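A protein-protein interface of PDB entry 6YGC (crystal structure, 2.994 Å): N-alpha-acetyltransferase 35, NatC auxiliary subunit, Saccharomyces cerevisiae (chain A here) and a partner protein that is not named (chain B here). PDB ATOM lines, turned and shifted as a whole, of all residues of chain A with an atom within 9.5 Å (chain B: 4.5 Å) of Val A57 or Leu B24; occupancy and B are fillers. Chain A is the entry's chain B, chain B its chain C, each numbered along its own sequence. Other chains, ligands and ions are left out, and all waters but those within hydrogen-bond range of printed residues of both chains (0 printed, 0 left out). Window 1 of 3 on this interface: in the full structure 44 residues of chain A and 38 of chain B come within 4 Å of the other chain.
Phe A18 touches none of the printed residues of chain B. Val A57 touches just these residues of chain B: Leu B18 (3.9 Å), Leu B24 (3.97 Å), Val B56 (3.7 Å), Ser B57 (3.2 Å), Val B58 (3.8 Å), Pro B59 (3.6 Å) and Ser B62 (3.7 Å). No residue of chain A comes within 4 Å of Val B16. Printed residues of chain A within 4 Å of Leu B18: Val A57 (3.9 Å). No residue of chain A comes within 4 Å of Ile B23. Of chain A, only Val A57 (3.97 Å) comes within 4 Å of Leu B24. Of the printed residues of chain A, Glu B44 touches Ser A65. Printed residues of chain A within 4 Å of Val B56: Leu A55 and Val A57. Of the printed residues of chain A, Ser B57 touches Leu A55 (2.4 Å), Glu A56 (3.3 Å) and Val A57 (3.2 Å). The nearest printed residue of chain B that does not touch Val A57 is Arg B22 (4.5 Å). The nearest residue of chain A that does not touch Leu B24 is Ser A65 (7.1 Å).
The backbone carbonyl oxygen (O) of Ser B57 sits at hydrogen-bond distance from the backbone NH (N) of Val A57 (3.2 Å). OG of Ser B62 sits at hydrogen-bond distance from OD1 of Asn A58 (3.0 Å). The side-chain carboxylate (OD2) of Asp A63 is in salt-bridge range of the guanidinium group (NH1) of Arg B22 (2.8 Å). NH2 of Arg B22 lies within hydrogen-bond range of OG of Ser A65, 2.9 Å away. O of Leu A55 lies close to N of Ser B57. The side-chain hydroxyl of Ser A65 lies close to the side-chain carboxylate of Glu B44, 2.3 Å away.
The side-chain amide nitrogen of Asn A59 is in hydrogen-bond range of the side-chain carboxylate of Glu A56 (3.2 Å). The backbone NH of Asn A58 sits at hydrogen-bond distance from the side-chain carboxylate of Asp A63 (2.8 Å). N of Ser A65 lies within hydrogen-bond range of OD1 of Asp A63, at 2.8 Å. N of Leu B24 lies within hydrogen-bond range of O of Val B16, at 2.8 Å. NH2 of Arg B22 is in salt-bridge range of OE2 of Glu B44.
Among the printed residues, merely in contact across the chains: Leu A55 with Val B56 (3.3 Å), Glu A56 with Ser B57 (3.3 Å), Glu A56 with Pro B59 (3.9 Å), Val A57 with Leu B18 (3.9 Å), Val A57 with Leu B24 (3.97 Å), Val A57 with Val B56 (3.7 Å), Val A57 with Val B58 (3.8 Å), Val A57 with Pro B59 (3.6 Å) and Val A57 with Ser B62 (3.7 Å).
Hydrophobic or aromatic side chains of chain B that line the printed part of chain A: Leu B18, Leu B24, Val B56, Val B58 and Pro B59. Of the 16 printed residues of chain A, 6 touch a printed residue of chain B. Among the printed residues, 15 pairs touch across the chains. Among the printed residues, Asp or Glu carboxylates within 4 Å of a Lys or Arg side-chain nitrogen of the other chain: Asp A63 with Arg B22.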
ATOM      1  N   ILE A  14      -4.324  34.472  12.674  1.00  0.00           N
ATOM      2  CA  ILE A  14      -3.173  34.187  11.822  1.00  0.00           C
ATOM      3  C   ILE A  14      -2.175  35.342  11.850  1.00  0.00           C
ATOM      4  O   ILE A  14      -0.961  35.126  11.747  1.00  0.00           O
ATOM      5  CB  ILE A  14      -3.639  33.866  10.387  1.00  0.00           C
ATOM      6  CG1 ILE A  14      -4.388  35.053   9.781  1.00  0.00           C
ATOM      7  CG2 ILE A  14      -4.524  32.620  10.382  1.00  0.00           C
ATOM      8  CD1 ILE A  14      -4.992  34.754   8.430  1.00  0.00           C
ATOM      9  N   PHE A  18       2.310  38.657  14.824  1.00  0.00           N
ATOM     10  CA  PHE A  18       3.044  39.843  14.404  1.00  0.00           C
ATOM     11  C   PHE A  18       2.287  41.097  14.829  1.00  0.00           C
ATOM     12  O   PHE A  18       1.096  41.240  14.534  1.00  0.00           O
ATOM     13  CB  PHE A  18       3.265  39.833  12.891  1.00  0.00           C
ATOM     14  CG  PHE A  18       4.018  38.630  12.402  1.00  0.00           C
ATOM     15  CD1 PHE A  18       5.402  38.596  12.451  1.00  0.00           C
ATOM     16  CD2 PHE A  18       3.343  37.531  11.899  1.00  0.00           C
ATOM     17  CE1 PHE A  18       6.098  37.489  12.004  1.00  0.00           C
ATOM     18  CE2 PHE A  18       4.032  36.424  11.452  1.00  0.00           C
ATOM     19  CZ  PHE A  18       5.411  36.402  11.504  1.00  0.00           C
ATOM     20  N   LEU A  21       2.195  45.183  10.665  1.00  0.00           N
ATOM     21  CA  LEU A  21       2.477  44.736   9.309  1.00  0.00           C
ATOM     22  C   LEU A  21       2.428  45.911   8.345  1.00  0.00           C
ATOM     23  O   LEU A  21       1.555  46.778   8.448  1.00  0.00           O
ATOM     24  CB  LEU A  21       1.490  43.653   8.856  1.00  0.00           C
ATOM     25  CG  LEU A  21       1.716  42.242   9.402  1.00  0.00           C
ATOM     26  CD1 LEU A  21       0.920  41.235   8.589  1.00  0.00           C
ATOM     27  CD2 LEU A  21       3.196  41.885   9.401  1.00  0.00           C
ATOM     28  N   SER A  54      12.587  22.975  -4.751  1.00  0.00           N
ATOM     29  CA  SER A  54      11.536  23.865  -4.292  1.00  0.00           C
ATOM     30  C   SER A  54      10.176  23.411  -4.804  1.00  0.00           C
ATOM     31  O   SER A  54      10.054  22.837  -5.891  1.00  0.00           O
ATOM     32  CB  SER A  54      11.805  25.297  -4.756  1.00  0.00           C
ATOM     33  OG  SER A  54      11.780  25.383  -6.170  1.00  0.00           O
ATOM     34  N   LEU A  55       9.150  23.666  -4.001  1.00  0.00           N
ATOM     35  CA  LEU A  55       7.773  23.475  -4.422  1.00  0.00           C
ATOM     36  C   LEU A  55       7.243  24.767  -5.035  1.00  0.00           C
ATOM     37  O   LEU A  55       7.769  25.855  -4.798  1.00  0.00           O
ATOM     38  CB  LEU A  55       6.897  23.053  -3.241  1.00  0.00           C
ATOM     39  CG  LEU A  55       7.395  21.890  -2.379  1.00  0.00           C
ATOM     40  CD1 LEU A  55       6.371  21.554  -1.306  1.00  0.00           C
ATOM     41  CD2 LEU A  55       7.704  20.671  -3.233  1.00  0.00           C
ATOM     42  N   GLU A  56       6.188  24.635  -5.834  1.00  0.00           N
ATOM     43  CA  GLU A  56       5.577  25.779  -6.498  1.00  0.00           C
ATOM     44  C   GLU A  56       4.089  25.804  -6.187  1.00  0.00           C
ATOM     45  O   GLU A  56       3.397  24.796  -6.365  1.00  0.00           O
ATOM     46  CB  GLU A  56       5.805  25.731  -8.012  1.00  0.00           C
ATOM     47  CG  GLU A  56       5.905  27.102  -8.656  1.00  0.00           C
ATOM     48  CD  GLU A  56       6.012  27.033 -10.166  1.00  0.00           C
ATOM     49  OE1 GLU A  56       5.078  26.506 -10.808  1.00  0.00           O
ATOM     50  OE2 GLU A  56       7.034  27.498 -10.709  1.00  0.00           O
ATOM     51  N   VAL A  57       3.600  26.955  -5.722  1.00  0.00           N
ATOM     52  CA  VAL A  57       2.189  27.080  -5.388  1.00  0.00           C
ATOM     53  C   VAL A  57       1.360  27.150  -6.665  1.00  0.00           C
ATOM     54  O   VAL A  57       1.828  27.604  -7.719  1.00  0.00           O
ATOM     55  CB  VAL A  57       1.943  28.310  -4.495  1.00  0.00           C
ATOM     56  CG1 VAL A  57       2.712  28.179  -3.189  1.00  0.00           C
ATOM     57  CG2 VAL A  57       2.334  29.584  -5.220  1.00  0.00           C
ATOM     58  N   ASN A  58       0.117  26.679  -6.571  1.00  0.00           N
ATOM     59  CA  ASN A  58      -0.832  26.636  -7.682  1.00  0.00           C
ATOM     60  C   ASN A  58      -0.328  25.797  -8.854  1.00  0.00           C
ATOM     61  O   ASN A  58      -0.823  25.932  -9.977  1.00  0.00           O
ATOM     62  CB  ASN A  58      -1.204  28.049  -8.150  1.00  0.00           C
ATOM     63  CG  ASN A  58      -1.957  28.830  -7.090  1.00  0.00           C
ATOM     64  OD1 ASN A  58      -1.565  29.937  -6.722  1.00  0.00           O
ATOM     65  ND2 ASN A  58      -3.040  28.250  -6.585  1.00  0.00           N
ATOM     66  N   ASN A  59       0.650  24.926  -8.608  1.00  0.00           N
ATOM     67  CA  ASN A  59       1.108  23.935  -9.577  1.00  0.00           C
ATOM     68  C   ASN A  59       0.597  22.581  -9.099  1.00  0.00           C
ATOM     69  O   ASN A  59       1.026  22.089  -8.049  1.00  0.00           O
ATOM     70  CB  ASN A  59       2.631  23.947  -9.703  1.00  0.00           C
ATOM     71  CG  ASN A  59       3.134  23.099 -10.862  1.00  0.00           C
ATOM     72  OD1 ASN A  59       2.486  22.137 -11.276  1.00  0.00           O
ATOM     73  ND2 ASN A  59       4.302  23.454 -11.387  1.00  0.00           N
ATOM     74  N   SER A  60      -0.316  21.984  -9.869  1.00  0.00           N
ATOM     75  CA  SER A  60      -0.983  20.761  -9.429  1.00  0.00           C
ATOM     76  C   SER A  60       0.021  19.655  -9.124  1.00  0.00           C
ATOM     77  O   SER A  60      -0.168  18.878  -8.181  1.00  0.00           O
ATOM     78  CB  SER A  60      -1.982  20.300 -10.490  1.00  0.00           C
ATOM     79  OG  SER A  60      -2.914  21.323 -10.793  1.00  0.00           O
ATOM     80  N   LYS A  61       1.098  19.576  -9.903  1.00  0.00           N
ATOM     81  CA  LYS A  61       2.101  18.537  -9.717  1.00  0.00           C
ATOM     82  C   LYS A  61       3.061  18.829  -8.570  1.00  0.00           C
ATOM     83  O   LYS A  61       3.789  17.922  -8.153  1.00  0.00           O
ATOM     84  CB  LYS A  61       2.893  18.341 -11.013  1.00  0.00           C
ATOM     85  CG  LYS A  61       2.017  18.182 -12.249  1.00  0.00           C
ATOM     86  CD  LYS A  61       2.844  18.088 -13.523  1.00  0.00           C
ATOM     87  CE  LYS A  61       3.645  16.798 -13.574  1.00  0.00           C
ATOM     88  NZ  LYS A  61       4.389  16.657 -14.857  1.00  0.00           N
ATOM     89  N   LEU A  62       3.074  20.056  -8.043  1.00  0.00           N
ATOM     90  CA  LEU A  62       4.017  20.429  -7.001  1.00  0.00           C
ATOM     91  C   LEU A  62       3.383  21.096  -5.785  1.00  0.00           C
ATOM     92  O   LEU A  62       4.111  21.447  -4.851  1.00  0.00           O
ATOM     93  CB  LEU A  62       5.098  21.365  -7.567  1.00  0.00           C
ATOM     94  CG  LEU A  62       6.141  20.749  -8.503  1.00  0.00           C
ATOM     95  CD1 LEU A  62       7.036  21.829  -9.091  1.00  0.00           C
ATOM     96  CD2 LEU A  62       6.973  19.714  -7.770  1.00  0.00           C
ATOM     97  N   ASP A  63       2.066  21.284  -5.762  1.00  0.00           N
ATOM     98  CA  ASP A  63       1.384  21.910  -4.634  1.00  0.00           C
ATOM     99  C   ASP A  63       0.575  20.852  -3.898  1.00  0.00           C
ATOM    100  O   ASP A  63      -0.340  20.252  -4.473  1.00  0.00           O
ATOM    101  CB  ASP A  63       0.481  23.054  -5.095  1.00  0.00           C
ATOM    102  CG  ASP A  63       0.058  23.964  -3.954  1.00  0.00           C
ATOM    103  OD1 ASP A  63       0.095  23.522  -2.785  1.00  0.00           O
ATOM    104  OD2 ASP A  63      -0.316  25.123  -4.226  1.00  0.00           O
ATOM    105  N   SER A  64       0.911  20.632  -2.627  1.00  0.00           N
ATOM    106  CA  SER A  64       0.177  19.673  -1.813  1.00  0.00           C
ATOM    107  C   SER A  64      -1.194  20.194  -1.402  1.00  0.00           C
ATOM    108  O   SER A  64      -2.066  19.395  -1.045  1.00  0.00           O
ATOM    109  CB  SER A  64       0.995  19.313  -0.574  1.00  0.00           C
ATOM    110  OG  SER A  64       0.271  18.446   0.276  1.00  0.00           O
ATOM    111  N   SER A  65      -1.406  21.510  -1.445  1.00  0.00           N
ATOM    112  CA  SER A  65      -2.682  22.080  -1.035  1.00  0.00           C
ATOM    113  C   SER A  65      -3.770  21.916  -2.088  1.00  0.00           C
ATOM    114  O   SER A  65      -4.954  22.058  -1.762  1.00  0.00           O
ATOM    115  CB  SER A  65      -2.512  23.565  -0.704  1.00  0.00           C
ATOM    116  OG  SER A  65      -1.552  23.751   0.320  1.00  0.00           O
ATOM    117  N   LEU A  66      -3.403  21.622  -3.333  1.00  0.00           N
ATOM    118  CA  LEU A  66      -4.365  21.495  -4.419  1.00  0.00           C
ATOM    119  C   LEU A  66      -4.871  20.071  -4.606  1.00  0.00           C
ATOM    120  O   LEU A  66      -5.554  19.798  -5.600  1.00  0.00           O
ATOM    121  CB  LEU A  66      -3.754  21.994  -5.729  1.00  0.00           C
ATOM    122  CG  LEU A  66      -3.259  23.438  -5.778  1.00  0.00           C
ATOM    123  CD1 LEU A  66      -2.975  23.834  -7.217  1.00  0.00           C
ATOM    124  CD2 LEU A  66      -4.263  24.385  -5.139  1.00  0.00           C
ATOM    125  N   LEU B  14       8.968  37.149   5.453  1.00  0.00           N
ATOM    126  CA  LEU B  14       7.937  37.876   4.729  1.00  0.00           C
ATOM    127  C   LEU B  14       6.607  37.147   4.872  1.00  0.00           C
ATOM    128  O   LEU B  14       6.563  35.913   4.877  1.00  0.00           O
ATOM    129  CB  LEU B  14       8.292  38.021   3.245  1.00  0.00           C
ATOM    130  CG  LEU B  14       9.619  38.707   2.917  1.00  0.00           C
ATOM    131  CD1 LEU B  14       9.745  38.932   1.417  1.00  0.00           C
ATOM    132  CD2 LEU B  14       9.751  40.017   3.675  1.00  0.00           C
ATOM    133  N   ILE B  15       5.530  37.915   4.994  1.00  0.00           N
ATOM    134  CA  ILE B  15       4.178  37.376   5.072  1.00  0.00           C
ATOM    135  C   ILE B  15       3.563  37.545   3.687  1.00  0.00           C
ATOM    136  O   ILE B  15       3.092  38.627   3.325  1.00  0.00           O
ATOM    137  CB  ILE B  15       3.345  38.064   6.159  1.00  0.00           C
ATOM    138  CG1 ILE B  15       3.865  37.696   7.553  1.00  0.00           C
ATOM    139  CG2 ILE B  15       1.874  37.686   6.033  1.00  0.00           C
ATOM    140  CD1 ILE B  15       5.032  38.538   8.032  1.00  0.00           C
ATOM    141  N   VAL B  16       3.581  36.472   2.906  1.00  0.00           N
ATOM    142  CA  VAL B  16       3.110  36.487   1.527  1.00  0.00           C
ATOM    143  C   VAL B  16       1.733  35.836   1.500  1.00  0.00           C
ATOM    144  O   VAL B  16       1.598  34.633   1.748  1.00  0.00           O
ATOM    145  CB  VAL B  16       4.085  35.764   0.591  1.00  0.00           C
ATOM    146  CG1 VAL B  16       3.614  35.875  -0.850  1.00  0.00           C
ATOM    147  CG2 VAL B  16       5.490  36.326   0.750  1.00  0.00           C
ATOM    148  N   LEU B  18      -1.256  34.387  -0.480  1.00  0.00           N
ATOM    149  CA  LEU B  18      -1.524  33.852  -1.805  1.00  0.00           C
ATOM    150  C   LEU B  18      -2.854  34.388  -2.334  1.00  0.00           C
ATOM    151  O   LEU B  18      -3.631  35.028  -1.620  1.00  0.00           O
ATOM    152  CB  LEU B  18      -1.522  32.324  -1.779  1.00  0.00           C
ATOM    153  CG  LEU B  18      -0.183  31.696  -1.382  1.00  0.00           C
ATOM    154  CD1 LEU B  18      -0.199  30.188  -1.583  1.00  0.00           C
ATOM    155  CD2 LEU B  18       0.956  32.335  -2.162  1.00  0.00           C
ATOM    156  N   ARG B  22      -4.698  31.965   1.230  1.00  0.00           N
ATOM    157  CA  ARG B  22      -3.566  31.200   1.734  1.00  0.00           C
ATOM    158  C   ARG B  22      -2.472  32.166   2.163  1.00  0.00           C
ATOM    159  O   ARG B  22      -2.190  33.144   1.466  1.00  0.00           O
ATOM    160  CB  ARG B  22      -3.023  30.226   0.680  1.00  0.00           C
ATOM    161  CG  ARG B  22      -4.015  29.172   0.219  1.00  0.00           C
ATOM    162  CD  ARG B  22      -3.404  28.282  -0.853  1.00  0.00           C
ATOM    163  NE  ARG B  22      -2.228  27.568  -0.366  1.00  0.00           N
ATOM    164  CZ  ARG B  22      -1.432  26.828  -1.132  1.00  0.00           C
ATOM    165  NH1 ARG B  22      -1.684  26.704  -2.428  1.00  0.00           N
ATOM    166  NH2 ARG B  22      -0.383  26.212  -0.603  1.00  0.00           N
ATOM    167  N   ILE B  23      -1.862  31.890   3.313  1.00  0.00           N
ATOM    168  CA  ILE B  23      -0.834  32.749   3.888  1.00  0.00           C
ATOM    169  C   ILE B  23       0.451  31.945   4.018  1.00  0.00           C
ATOM    170  O   ILE B  23       0.455  30.860   4.610  1.00  0.00           O
ATOM    171  CB  ILE B  23      -1.261  33.312   5.257  1.00  0.00           C
ATOM    172  CG1 ILE B  23      -2.645  33.957   5.165  1.00  0.00           C
ATOM    173  CG2 ILE B  23      -0.234  34.314   5.764  1.00  0.00           C
ATOM    174  CD1 ILE B  23      -2.720  35.111   4.194  1.00  0.00           C
ATOM    175  N   LEU B  24       1.539  32.479   3.468  1.00  0.00           N
ATOM    176  CA  LEU B  24       2.855  31.861   3.546  1.00  0.00           C
ATOM    177  C   LEU B  24       3.778  32.738   4.380  1.00  0.00           C
ATOM    178  O   LEU B  24       3.935  33.931   4.094  1.00  0.00           O
ATOM    179  CB  LEU B  24       3.450  31.650   2.151  1.00  0.00           C
ATOM    180  CG  LEU B  24       2.728  30.683   1.213  1.00  0.00           C
ATOM    181  CD1 LEU B  24       3.487  30.550  -0.098  1.00  0.00           C
ATOM    182  CD2 LEU B  24       2.551  29.325   1.874  1.00  0.00           C
ATOM    183  N   VAL B  25       4.385  32.149   5.406  1.00  0.00           N
ATOM    184  CA  VAL B  25       5.309  32.847   6.293  1.00  0.00           C
ATOM    185  C   VAL B  25       6.651  32.133   6.204  1.00  0.00           C
ATOM    186  O   VAL B  25       6.783  30.988   6.655  1.00  0.00           O
ATOM    187  CB  VAL B  25       4.799  32.889   7.739  1.00  0.00           C
ATOM    188  CG1 VAL B  25       5.806  33.589   8.639  1.00  0.00           C
ATOM    189  CG2 VAL B  25       3.447  33.583   7.806  1.00  0.00           C
ATOM    190  N   GLY B  26       7.641  32.801   5.622  1.00  0.00           N
ATOM    191  CA  GLY B  26       8.956  32.209   5.470  1.00  0.00           C
ATOM    192  C   GLY B  26       9.977  33.248   5.070  1.00  0.00           C
ATOM    193  O   GLY B  26       9.634  34.355   4.641  1.00  0.00           O
ATOM    194  N   VAL B  42       8.975  27.777   5.089  1.00  0.00           N
ATOM    195  CA  VAL B  42       7.638  28.300   4.847  1.00  0.00           C
ATOM    196  C   VAL B  42       6.649  27.664   5.812  1.00  0.00           C
ATOM    197  O   VAL B  42       6.650  26.444   6.017  1.00  0.00           O
ATOM    198  CB  VAL B  42       7.225  28.056   3.388  1.00  0.00           C
ATOM    199  CG1 VAL B  42       5.709  27.989   3.254  1.00  0.00           C
ATOM    200  CG2 VAL B  42       7.780  29.147   2.501  1.00  0.00           C
ATOM    201  N   GLU B  43       5.803  28.495   6.416  1.00  0.00           N
ATOM    202  CA  GLU B  43       4.665  28.041   7.204  1.00  0.00           C
ATOM    203  C   GLU B  43       3.393  28.437   6.466  1.00  0.00           C
ATOM    204  O   GLU B  43       3.162  29.625   6.216  1.00  0.00           O
ATOM    205  CB  GLU B  43       4.688  28.647   8.608  1.00  0.00           C
ATOM    206  CG  GLU B  43       3.574  28.146   9.510  1.00  0.00           C
ATOM    207  CD  GLU B  43       3.557  28.841  10.856  1.00  0.00           C
ATOM    208  OE1 GLU B  43       4.266  29.858  11.011  1.00  0.00           O
ATOM    209  OE2 GLU B  43       2.836  28.369  11.759  1.00  0.00           O
ATOM    210  N   GLU B  44       2.578  27.445   6.114  1.00  0.00           N
ATOM    211  CA  GLU B  44       1.352  27.665   5.354  1.00  0.00           C
ATOM    212  C   GLU B  44       0.181  27.763   6.327  1.00  0.00           C
ATOM    213  O   GLU B  44      -0.182  26.776   6.974  1.00  0.00           O
ATOM    214  CB  GLU B  44       1.129  26.539   4.346  1.00  0.00           C
ATOM    215  CG  GLU B  44      -0.050  26.765   3.416  1.00  0.00           C
ATOM    216  CD  GLU B  44      -0.897  25.521   3.237  1.00  0.00           C
ATOM    217  OE1 GLU B  44      -1.126  24.807   4.236  1.00  0.00           O
ATOM    218  OE2 GLU B  44      -1.330  25.254   2.097  1.00  0.00           O
ATOM    219  N   VAL B  56       9.656  26.731  -0.735  1.00  0.00           N
ATOM    220  CA  VAL B  56       8.550  26.901  -1.669  1.00  0.00           C
ATOM    221  C   VAL B  56       8.867  28.057  -2.610  1.00  0.00           C
ATOM    222  O   VAL B  56       9.489  29.049  -2.219  1.00  0.00           O
ATOM    223  CB  VAL B  56       7.212  27.150  -0.937  1.00  0.00           C
ATOM    224  CG1 VAL B  56       6.047  27.099  -1.911  1.00  0.00           C
ATOM    225  CG2 VAL B  56       7.017  26.143   0.185  1.00  0.00           C
ATOM    226  N   SER B  57       8.434  27.920  -3.859  1.00  0.00           N
ATOM    227  CA  SER B  57       8.556  28.967  -4.862  1.00  0.00           C
ATOM    228  C   SER B  57       7.187  29.559  -5.151  1.00  0.00           C
ATOM    229  O   SER B  57       6.210  28.826  -5.331  1.00  0.00           O
ATOM    230  CB  SER B  57       9.170  28.428  -6.158  1.00  0.00           C
ATOM    231  OG  SER B  57       9.208  29.440  -7.148  1.00  0.00           O
ATOM    232  N   VAL B  58       7.119  30.886  -5.199  1.00  0.00           N
ATOM    233  CA  VAL B  58       5.847  31.576  -5.417  1.00  0.00           C
ATOM    234  C   VAL B  58       5.921  32.388  -6.705  1.00  0.00           C
ATOM    235  O   VAL B  58       6.710  33.339  -6.788  1.00  0.00           O
ATOM    236  CB  VAL B  58       5.493  32.470  -4.218  1.00  0.00           C
ATOM    237  CG1 VAL B  58       4.011  32.792  -4.220  1.00  0.00           C
ATOM    238  CG2 VAL B  58       5.896  31.812  -2.910  1.00  0.00           C
ATOM    239  N   PRO B  59       5.144  32.046  -7.729  1.00  0.00           N
ATOM    240  CA  PRO B  59       5.115  32.868  -8.944  1.00  0.00           C
ATOM    241  C   PRO B  59       4.434  34.205  -8.691  1.00  0.00           C
ATOM    242  O   PRO B  59       3.757  34.418  -7.684  1.00  0.00           O
ATOM    243  CB  PRO B  59       4.315  32.014  -9.935  1.00  0.00           C
ATOM    244  CG  PRO B  59       4.384  30.619  -9.390  1.00  0.00           C
ATOM    245  CD  PRO B  59       4.407  30.783  -7.905  1.00  0.00           C
ATOM    246  N   SER B  62       0.487  34.186  -8.550  1.00  0.00           N
ATOM    247  CA  SER B  62      -0.092  33.583  -7.355  1.00  0.00           C
ATOM    248  C   SER B  62      -0.086  34.529  -6.162  1.00  0.00           C
ATOM    249  O   SER B  62      -0.856  34.319  -5.218  1.00  0.00           O
ATOM    250  CB  SER B  62       0.660  32.300  -7.000  1.00  0.00           C
ATOM    251  OG  SER B  62       0.703  31.409  -8.101  1.00  0.00           O
